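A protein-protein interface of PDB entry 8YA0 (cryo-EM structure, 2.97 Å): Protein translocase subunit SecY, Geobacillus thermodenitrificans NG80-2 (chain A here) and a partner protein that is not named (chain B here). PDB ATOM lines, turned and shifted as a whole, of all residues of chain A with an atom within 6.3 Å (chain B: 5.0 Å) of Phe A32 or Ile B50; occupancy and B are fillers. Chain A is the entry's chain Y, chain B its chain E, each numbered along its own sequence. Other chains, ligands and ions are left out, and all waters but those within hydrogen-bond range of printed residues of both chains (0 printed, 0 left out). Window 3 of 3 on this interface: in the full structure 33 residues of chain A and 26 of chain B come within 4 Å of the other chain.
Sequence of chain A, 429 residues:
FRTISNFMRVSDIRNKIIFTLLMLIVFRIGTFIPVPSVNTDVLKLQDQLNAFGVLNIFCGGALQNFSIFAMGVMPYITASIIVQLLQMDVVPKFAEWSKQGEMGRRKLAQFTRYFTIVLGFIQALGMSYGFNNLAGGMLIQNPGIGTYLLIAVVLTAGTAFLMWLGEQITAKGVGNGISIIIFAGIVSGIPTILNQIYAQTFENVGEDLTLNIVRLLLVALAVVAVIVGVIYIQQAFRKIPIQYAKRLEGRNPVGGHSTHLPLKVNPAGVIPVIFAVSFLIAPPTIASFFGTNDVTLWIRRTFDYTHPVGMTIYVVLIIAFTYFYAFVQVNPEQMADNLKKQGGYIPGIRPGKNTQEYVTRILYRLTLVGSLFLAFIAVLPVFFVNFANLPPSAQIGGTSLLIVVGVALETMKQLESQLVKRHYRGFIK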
ATOM      1  N   ILE A  25      28.269 -36.452 -25.405  1.00  0.00           N
ATOM      2  CA  ILE A  25      27.579 -35.531 -24.504  1.00  0.00           C
ATOM      3  C   ILE A  25      27.951 -34.089 -24.827  1.00  0.00           C
ATOM      4  O   ILE A  25      27.094 -33.203 -24.803  1.00  0.00           O
ATOM      5  CB  ILE A  25      27.883 -35.896 -23.041  1.00  0.00           C
ATOM      6  CG1 ILE A  25      27.164 -37.181 -22.665  1.00  0.00           C
ATOM      7  CG2 ILE A  25      27.432 -34.822 -22.090  1.00  0.00           C
ATOM      8  CD1 ILE A  25      27.411 -37.620 -21.256  1.00  0.00           C
ATOM      9  N   PHE A  27      28.800 -32.956 -27.825  1.00  0.00           N
ATOM     10  CA  PHE A  27      28.076 -32.659 -29.059  1.00  0.00           C
ATOM     11  C   PHE A  27      26.613 -32.322 -28.788  1.00  0.00           C
ATOM     12  O   PHE A  27      26.079 -31.354 -29.340  1.00  0.00           O
ATOM     13  CB  PHE A  27      28.217 -33.850 -30.009  1.00  0.00           C
ATOM     14  CG  PHE A  27      27.148 -33.947 -31.049  1.00  0.00           C
ATOM     15  CD1 PHE A  27      27.166 -33.132 -32.151  1.00  0.00           C
ATOM     16  CD2 PHE A  27      26.147 -34.887 -30.943  1.00  0.00           C
ATOM     17  CE1 PHE A  27      26.200 -33.226 -33.103  1.00  0.00           C
ATOM     18  CE2 PHE A  27      25.180 -34.978 -31.890  1.00  0.00           C
ATOM     19  CZ  PHE A  27      25.210 -34.147 -32.973  1.00  0.00           C
ATOM     20  N   ARG A  28      25.970 -33.061 -27.889  1.00  0.00           N
ATOM     21  CA  ARG A  28      24.569 -32.793 -27.583  1.00  0.00           C
ATOM     22  C   ARG A  28      24.390 -31.483 -26.816  1.00  0.00           C
ATOM     23  O   ARG A  28      23.428 -30.730 -27.061  1.00  0.00           O
ATOM     24  CB  ARG A  28      24.008 -33.957 -26.791  1.00  0.00           C
ATOM     25  CG  ARG A  28      22.539 -34.044 -26.833  1.00  0.00           C
ATOM     26  CD  ARG A  28      22.080 -34.719 -28.084  1.00  0.00           C
ATOM     27  NE  ARG A  28      20.628 -34.779 -28.133  1.00  0.00           N
ATOM     28  CZ  ARG A  28      19.891 -34.099 -28.997  1.00  0.00           C
ATOM     29  NH1 ARG A  28      20.470 -33.319 -29.890  1.00  0.00           N
ATOM     30  NH2 ARG A  28      18.575 -34.212 -28.975  1.00  0.00           N
ATOM     31  N   ILE A  29      25.313 -31.204 -25.890  1.00  0.00           N
ATOM     32  CA  ILE A  29      25.324 -29.954 -25.133  1.00  0.00           C
ATOM     33  C   ILE A  29      25.414 -28.775 -26.077  1.00  0.00           C
ATOM     34  O   ILE A  29      24.670 -27.801 -25.945  1.00  0.00           O
ATOM     35  CB  ILE A  29      26.492 -29.959 -24.127  1.00  0.00           C
ATOM     36  CG1 ILE A  29      26.113 -30.682 -22.847  1.00  0.00           C
ATOM     37  CG2 ILE A  29      26.933 -28.566 -23.762  1.00  0.00           C
ATOM     38  CD1 ILE A  29      27.278 -30.955 -21.959  1.00  0.00           C
ATOM     39  N   GLY A  30      26.284 -28.868 -27.077  1.00  0.00           N
ATOM     40  CA  GLY A  30      26.386 -27.789 -28.037  1.00  0.00           C
ATOM     41  C   GLY A  30      25.186 -27.685 -28.953  1.00  0.00           C
ATOM     42  O   GLY A  30      24.851 -26.597 -29.417  1.00  0.00           O
ATOM     43  N   THR A  31      24.507 -28.800 -29.203  1.00  0.00           N
ATOM     44  CA  THR A  31      23.272 -28.783 -29.979  1.00  0.00           C
ATOM     45  C   THR A  31      22.125 -28.135 -29.203  1.00  0.00           C
ATOM     46  O   THR A  31      21.113 -27.749 -29.791  1.00  0.00           O
ATOM     47  CB  THR A  31      23.008 -30.236 -30.413  1.00  0.00           C
ATOM     48  OG1 THR A  31      24.055 -30.630 -31.298  1.00  0.00           O
ATOM     49  CG2 THR A  31      21.735 -30.445 -31.184  1.00  0.00           C
ATOM     50  N   PHE A  32      22.278 -27.921 -27.902  1.00  0.00           N
ATOM     51  CA  PHE A  32      21.286 -27.102 -27.206  1.00  0.00           C
ATOM     52  C   PHE A  32      21.559 -25.596 -27.223  1.00  0.00           C
ATOM     53  O   PHE A  32      20.695 -24.833 -26.792  1.00  0.00           O
ATOM     54  CB  PHE A  32      21.152 -27.563 -25.761  1.00  0.00           C
ATOM     55  CG  PHE A  32      20.029 -28.500 -25.552  1.00  0.00           C
ATOM     56  CD1 PHE A  32      18.773 -28.031 -25.270  1.00  0.00           C
ATOM     57  CD2 PHE A  32      20.221 -29.854 -25.671  1.00  0.00           C
ATOM     58  CE1 PHE A  32      17.736 -28.896 -25.093  1.00  0.00           C
ATOM     59  CE2 PHE A  32      19.186 -30.719 -25.500  1.00  0.00           C
ATOM     60  CZ  PHE A  32      17.944 -30.242 -25.207  1.00  0.00           C
ATOM     61  N   ILE A  33      22.708 -25.148 -27.720  1.00  0.00           N
ATOM     62  CA  ILE A  33      23.138 -23.757 -27.592  1.00  0.00           C
ATOM     63  C   ILE A  33      22.669 -22.988 -28.825  1.00  0.00           C
ATOM     64  O   ILE A  33      23.036 -23.365 -29.942  1.00  0.00           O
ATOM     65  CB  ILE A  33      24.660 -23.672 -27.457  1.00  0.00           C
ATOM     66  CG1 ILE A  33      25.104 -24.144 -26.085  1.00  0.00           C
ATOM     67  CG2 ILE A  33      25.150 -22.276 -27.690  1.00  0.00           C
ATOM     68  CD1 ILE A  33      26.584 -24.259 -25.966  1.00  0.00           C
ATOM     69  N   PRO A  34      21.923 -21.900 -28.673  1.00  0.00           N
ATOM     70  CA  PRO A  34      21.397 -21.193 -29.842  1.00  0.00           C
ATOM     71  C   PRO A  34      22.465 -20.367 -30.544  1.00  0.00           C
ATOM     72  O   PRO A  34      23.588 -20.211 -30.076  1.00  0.00           O
ATOM     73  CB  PRO A  34      20.319 -20.297 -29.247  1.00  0.00           C
ATOM     74  CG  PRO A  34      20.802 -20.022 -27.912  1.00  0.00           C
ATOM     75  CD  PRO A  34      21.484 -21.263 -27.429  1.00  0.00           C
ATOM     76  N   PHE A  52      11.204 -31.738 -29.170  1.00  0.00           N
ATOM     77  CA  PHE A  52      11.747 -31.501 -27.844  1.00  0.00           C
ATOM     78  C   PHE A  52      12.873 -30.482 -27.921  1.00  0.00           C
ATOM     79  O   PHE A  52      13.760 -30.588 -28.768  1.00  0.00           O
ATOM     80  CB  PHE A  52      12.260 -32.791 -27.213  1.00  0.00           C
ATOM     81  CG  PHE A  52      12.711 -32.623 -25.800  1.00  0.00           C
ATOM     82  CD1 PHE A  52      11.790 -32.401 -24.794  1.00  0.00           C
ATOM     83  CD2 PHE A  52      14.053 -32.670 -25.477  1.00  0.00           C
ATOM     84  CE1 PHE A  52      12.197 -32.238 -23.496  1.00  0.00           C
ATOM     85  CE2 PHE A  52      14.465 -32.504 -24.181  1.00  0.00           C
ATOM     86  CZ  PHE A  52      13.537 -32.290 -23.191  1.00  0.00           C
ATOM     87  N   GLY A  53      12.845 -29.514 -27.022  1.00  0.00           N
ATOM     88  CA  GLY A  53      13.766 -28.397 -27.076  1.00  0.00           C
ATOM     89  C   GLY A  53      13.110 -27.196 -27.714  1.00  0.00           C
ATOM     90  O   GLY A  53      11.938 -27.212 -28.089  1.00  0.00           O
ATOM     91  N   VAL A  54      13.881 -26.121 -27.822  1.00  0.00           N
ATOM     92  CA  VAL A  54      13.431 -24.939 -28.542  1.00  0.00           C
ATOM     93  C   VAL A  54      14.127 -24.795 -29.885  1.00  0.00           C
ATOM     94  O   VAL A  54      13.574 -24.147 -30.785  1.00  0.00           O
ATOM     95  CB  VAL A  54      13.593 -23.656 -27.692  1.00  0.00           C
ATOM     96  CG1 VAL A  54      15.001 -23.124 -27.732  1.00  0.00           C
ATOM     97  CG2 VAL A  54      12.632 -22.588 -28.130  1.00  0.00           C
ATOM     98  N   LEU A  55      15.280 -25.415 -30.078  1.00  0.00           N
ATOM     99  CA  LEU A  55      15.976 -25.320 -31.342  1.00  0.00           C
ATOM    100  C   LEU A  55      15.628 -26.451 -32.286  1.00  0.00           C
ATOM    101  O   LEU A  55      16.068 -26.436 -33.433  1.00  0.00           O
ATOM    102  CB  LEU A  55      17.474 -25.283 -31.102  1.00  0.00           C
ATOM    103  CG  LEU A  55      17.847 -24.222 -30.085  1.00  0.00           C
ATOM    104  CD1 LEU A  55      19.300 -24.324 -29.792  1.00  0.00           C
ATOM    105  CD2 LEU A  55      17.514 -22.859 -30.612  1.00  0.00           C
ATOM    106  N   ASN A  56      14.848 -27.420 -31.838  1.00  0.00           N
ATOM    107  CA  ASN A  56      14.448 -28.540 -32.666  1.00  0.00           C
ATOM    108  C   ASN A  56      13.039 -28.285 -33.160  1.00  0.00           C
ATOM    109  O   ASN A  56      12.136 -28.045 -32.359  1.00  0.00           O
ATOM    110  CB  ASN A  56      14.506 -29.846 -31.884  1.00  0.00           C
ATOM    111  CG  ASN A  56      15.846 -30.078 -31.251  1.00  0.00           C
ATOM    112  OD1 ASN A  56      16.877 -29.728 -31.811  1.00  0.00           O
ATOM    113  ND2 ASN A  56      15.842 -30.677 -30.075  1.00  0.00           N
ATOM    114  N   ASN A  65      17.166 -28.475 -36.944  1.00  0.00           N
ATOM    115  CA  ASN A  65      17.816 -27.973 -35.750  1.00  0.00           C
ATOM    116  C   ASN A  65      18.591 -26.722 -36.112  1.00  0.00           C
ATOM    117  O   ASN A  65      19.273 -26.695 -37.137  1.00  0.00           O
ATOM    118  CB  ASN A  65      18.740 -29.028 -35.162  1.00  0.00           C
ATOM    119  CG  ASN A  65      19.457 -28.546 -33.953  1.00  0.00           C
ATOM    120  OD1 ASN A  65      20.638 -28.236 -34.007  1.00  0.00           O
ATOM    121  ND2 ASN A  65      18.750 -28.472 -32.843  1.00  0.00           N
ATOM    122  N   SER A  67      20.789 -24.807 -33.895  1.00  0.00           N
ATOM    123  CA  SER A  67      21.783 -24.466 -32.897  1.00  0.00           C
ATOM    124  C   SER A  67      23.066 -24.044 -33.591  1.00  0.00           C
ATOM    125  O   SER A  67      23.080 -23.792 -34.791  1.00  0.00           O
ATOM    126  CB  SER A  67      22.031 -25.649 -31.999  1.00  0.00           C
ATOM    127  OG  SER A  67      21.958 -26.837 -32.747  1.00  0.00           O
ATOM    128  N   PHE A  69      25.384 -26.076 -34.054  1.00  0.00           N
ATOM    129  CA  PHE A  69      25.660 -27.269 -34.834  1.00  0.00           C
ATOM    130  C   PHE A  69      24.581 -27.524 -35.864  1.00  0.00           C
ATOM    131  O   PHE A  69      24.250 -28.678 -36.127  1.00  0.00           O
ATOM    132  CB  PHE A  69      25.782 -28.477 -33.920  1.00  0.00           C
ATOM    133  CG  PHE A  69      26.950 -28.430 -33.012  1.00  0.00           C
ATOM    134  CD1 PHE A  69      28.122 -27.836 -33.401  1.00  0.00           C
ATOM    135  CD2 PHE A  69      26.877 -28.988 -31.764  1.00  0.00           C
ATOM    136  CE1 PHE A  69      29.197 -27.805 -32.557  1.00  0.00           C
ATOM    137  CE2 PHE A  69      27.952 -28.962 -30.933  1.00  0.00           C
ATOM    138  CZ  PHE A  69      29.101 -28.366 -31.323  1.00  0.00           C
ATOM    139  N   ILE B  46      20.311 -37.953 -21.664  1.00  0.00           N
ATOM    140  CA  ILE B  46      21.081 -36.717 -21.598  1.00  0.00           C
ATOM    141  C   ILE B  46      20.337 -35.524 -22.190  1.00  0.00           C
ATOM    142  O   ILE B  46      20.629 -34.398 -21.793  1.00  0.00           O
ATOM    143  CB  ILE B  46      22.468 -36.843 -22.239  1.00  0.00           C
ATOM    144  CG1 ILE B  46      22.375 -37.021 -23.735  1.00  0.00           C
ATOM    145  CG2 ILE B  46      23.223 -37.985 -21.637  1.00  0.00           C
ATOM    146  CD1 ILE B  46      23.703 -36.882 -24.391  1.00  0.00           C
ATOM    147  N   ASP B  47      19.341 -35.716 -23.067  1.00  0.00           N
ATOM    148  CA  ASP B  47      18.477 -34.592 -23.424  1.00  0.00           C
ATOM    149  C   ASP B  47      17.643 -34.141 -22.243  1.00  0.00           C
ATOM    150  O   ASP B  47      17.485 -32.936 -22.026  1.00  0.00           O
ATOM    151  CB  ASP B  47      17.561 -34.929 -24.595  1.00  0.00           C
ATOM    152  CG  ASP B  47      18.306 -35.069 -25.902  1.00  0.00           C
ATOM    153  OD1 ASP B  47      19.503 -34.740 -25.936  1.00  0.00           O
ATOM    154  OD2 ASP B  47      17.696 -35.502 -26.905  1.00  0.00           O
ATOM    155  N   LEU B  48      17.130 -35.087 -21.448  1.00  0.00           N
ATOM    156  CA  LEU B  48      16.403 -34.718 -20.234  1.00  0.00           C
ATOM    157  C   LEU B  48      17.310 -34.026 -19.222  1.00  0.00           C
ATOM    158  O   LEU B  48      16.906 -33.050 -18.581  1.00  0.00           O
ATOM    159  CB  LEU B  48      15.768 -35.953 -19.610  1.00  0.00           C
ATOM    160  CG  LEU B  48      14.678 -36.648 -20.417  1.00  0.00           C
ATOM    161  CD1 LEU B  48      14.268 -37.922 -19.725  1.00  0.00           C
ATOM    162  CD2 LEU B  48      13.480 -35.752 -20.617  1.00  0.00           C
ATOM    163  N   GLY B  49      18.554 -34.483 -19.110  1.00  0.00           N
ATOM    164  CA  GLY B  49      19.472 -33.884 -18.155  1.00  0.00           C
ATOM    165  C   GLY B  49      19.904 -32.484 -18.544  1.00  0.00           C
ATOM    166  O   GLY B  49      19.915 -31.574 -17.711  1.00  0.00           O
ATOM    167  N   ILE B  50      20.265 -32.290 -19.815  1.00  0.00           N
ATOM    168  CA  ILE B  50      20.620 -30.963 -20.301  1.00  0.00           C
ATOM    169  C   ILE B  50      19.417 -30.038 -20.248  1.00  0.00           C
ATOM    170  O   ILE B  50      19.559 -28.855 -19.943  1.00  0.00           O
ATOM    171  CB  ILE B  50      21.216 -31.059 -21.719  1.00  0.00           C
ATOM    172  CG1 ILE B  50      22.539 -31.804 -21.702  1.00  0.00           C
ATOM    173  CG2 ILE B  50      21.530 -29.713 -22.285  1.00  0.00           C
ATOM    174  CD1 ILE B  50      22.887 -32.368 -23.040  1.00  0.00           C
ATOM    175  N   SER B  51      18.211 -30.566 -20.455  1.00  0.00           N
ATOM    176  CA  SER B  51      17.028 -29.722 -20.369  1.00  0.00           C
ATOM    177  C   SER B  51      16.758 -29.263 -18.941  1.00  0.00           C
ATOM    178  O   SER B  51      16.380 -28.107 -18.724  1.00  0.00           O
ATOM    179  CB  SER B  51      15.821 -30.459 -20.927  1.00  0.00           C
ATOM    180  OG  SER B  51      14.654 -30.085 -20.225  1.00  0.00           O
ATOM    181  N   GLN B  52      16.981 -30.133 -17.947  1.00  0.00           N
ATOM    182  CA  GLN B  52      16.790 -29.699 -16.564  1.00  0.00           C
ATOM    183  C   GLN B  52      17.871 -28.720 -16.125  1.00  0.00           C
ATOM    184  O   GLN B  52      17.577 -27.741 -15.432  1.00  0.00           O
ATOM    185  CB  GLN B  52      16.757 -30.891 -15.620  1.00  0.00           C
ATOM    186  CG  GLN B  52      15.594 -31.819 -15.837  1.00  0.00           C
ATOM    187  CD  GLN B  52      14.309 -31.092 -16.123  1.00  0.00           C
ATOM    188  OE1 GLN B  52      13.803 -30.344 -15.288  1.00  0.00           O
ATOM    189  NE2 GLN B  52      13.765 -31.308 -17.309  1.00  0.00           N
ATOM    190  N   LEU B  53      19.119 -28.953 -16.526  1.00  0.00           N
ATOM    191  CA  LEU B  53      20.190 -28.013 -16.205  1.00  0.00           C
ATOM    192  C   LEU B  53      19.996 -26.669 -16.897  1.00  0.00           C
ATOM    193  O   LEU B  53      20.354 -25.625 -16.342  1.00  0.00           O
ATOM    194  CB  LEU B  53      21.528 -28.625 -16.601  1.00  0.00           C
ATOM    195  CG  LEU B  53      22.837 -27.902 -16.323  1.00  0.00           C
ATOM    196  CD1 LEU B  53      23.828 -28.904 -15.788  1.00  0.00           C
ATOM    197  CD2 LEU B  53      23.389 -27.246 -17.573  1.00  0.00           C
ATOM    198  N   ILE B  54      19.423 -26.678 -18.099  1.00  0.00           N
ATOM    199  CA  ILE B  54      19.125 -25.449 -18.820  1.00  0.00           C
ATOM    200  C   ILE B  54      17.971 -24.717 -18.151  1.00  0.00           C
ATOM    201  O   ILE B  54      17.970 -23.486 -18.055  1.00  0.00           O
ATOM    202  CB  ILE B  54      18.842 -25.793 -20.296  1.00  0.00           C
ATOM    203  CG1 ILE B  54      20.141 -25.862 -21.092  1.00  0.00           C
ATOM    204  CG2 ILE B  54      17.898 -24.822 -20.954  1.00  0.00           C
ATOM    205  CD1 ILE B  54      20.893 -24.593 -21.103  1.00  0.00           C
ATOM    206  N   ARG B  55      16.993 -25.463 -17.637  1.00  0.00           N
ATOM    207  CA  ARG B  55      15.924 -24.848 -16.865  1.00  0.00           C
ATOM    208  C   ARG B  55      16.437 -24.268 -15.555  1.00  0.00           C
ATOM    209  O   ARG B  55      15.880 -23.293 -15.052  1.00  0.00           O
ATOM    210  CB  ARG B  55      14.825 -25.867 -16.590  1.00  0.00           C
ATOM    211  CG  ARG B  55      13.525 -25.255 -16.141  1.00  0.00           C
ATOM    212  CD  ARG B  55      12.566 -26.309 -15.654  1.00  0.00           C
ATOM    213  NE  ARG B  55      12.388 -27.368 -16.638  1.00  0.00           N
ATOM    214  CZ  ARG B  55      11.512 -27.321 -17.634  1.00  0.00           C
ATOM    215  NH1 ARG B  55      10.730 -26.260 -17.782  1.00  0.00           N
ATOM    216  NH2 ARG B  55      11.419 -28.333 -18.483  1.00  0.00           N
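Among the printed residues, pairs that only touch across the chains: Phe A32 with Ile B50 (3.6 Å), Ile A29 with Ile B50 (3.6 Å), Phe A52 with Ser B51 (3.7 Å), Phe A52 with Asp B47 (3.7 Å), Arg A28 with Ile B46 (3.8 Å) and Ile A25 with Ile B46 (3.9 Å).
Of chain B, only Ile B50 comes within 4 Å of Phe A32.
Ile B50 touches just these residues of chain A: Ile A29 (3.6 Å) and Phe A32 (3.6 Å).
Printed residues of chain B within 4 Å of Ile A29: Ile B50 (3.6 Å).
Of the printed residues of chain A, Asp B47 touches Arg A28 (2.5 Å) and Phe A52 (3.7 Å).
Of the printed residues of chain B, Ile A25 touches Ile B46.
Of the printed residues of chain B, Phe A52 touches Asp B47 and Ser B51.
Of the printed residues of chain A, Ile B46 touches Ile A25 (3.9 Å) and Arg A28 (3.8 Å).
Val A54 touches none of the printed residues of chain B.
Arg B55 touches none of the printed residues of chain A.
The nearest residue of chain B that does not touch Phe A32 is Asp B47 (4.1 Å).
The nearest residue of chain A that does not touch Ile B50 is Arg A28 (4.2 Å).
NE of Arg A28 lies within salt-bridge range of OD1 of Asp B47 (2.5 Å).
Hydrophobic or aromatic side chains of chain B within 4 Å of the printed part of chain A: Ile B46 and Ile B50.
Along chain B the printed residues that touch a printed residue of chain A span positions 46 to 51.
Printed residues of chain A that touch a printed residue of chain B: Ile A25, Arg A28, Ile A29, Phe A32 and Phe A52.
Among the printed residues, 7 pairs touch across the chains.
O of Phe A52 sits at hydrogen-bond distance from ND2 of Asn A56 (2.5 Å).
OG of Ser B51 lies within hydrogen-bond range of NE2 of Gln B52, 3.3 Å away.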
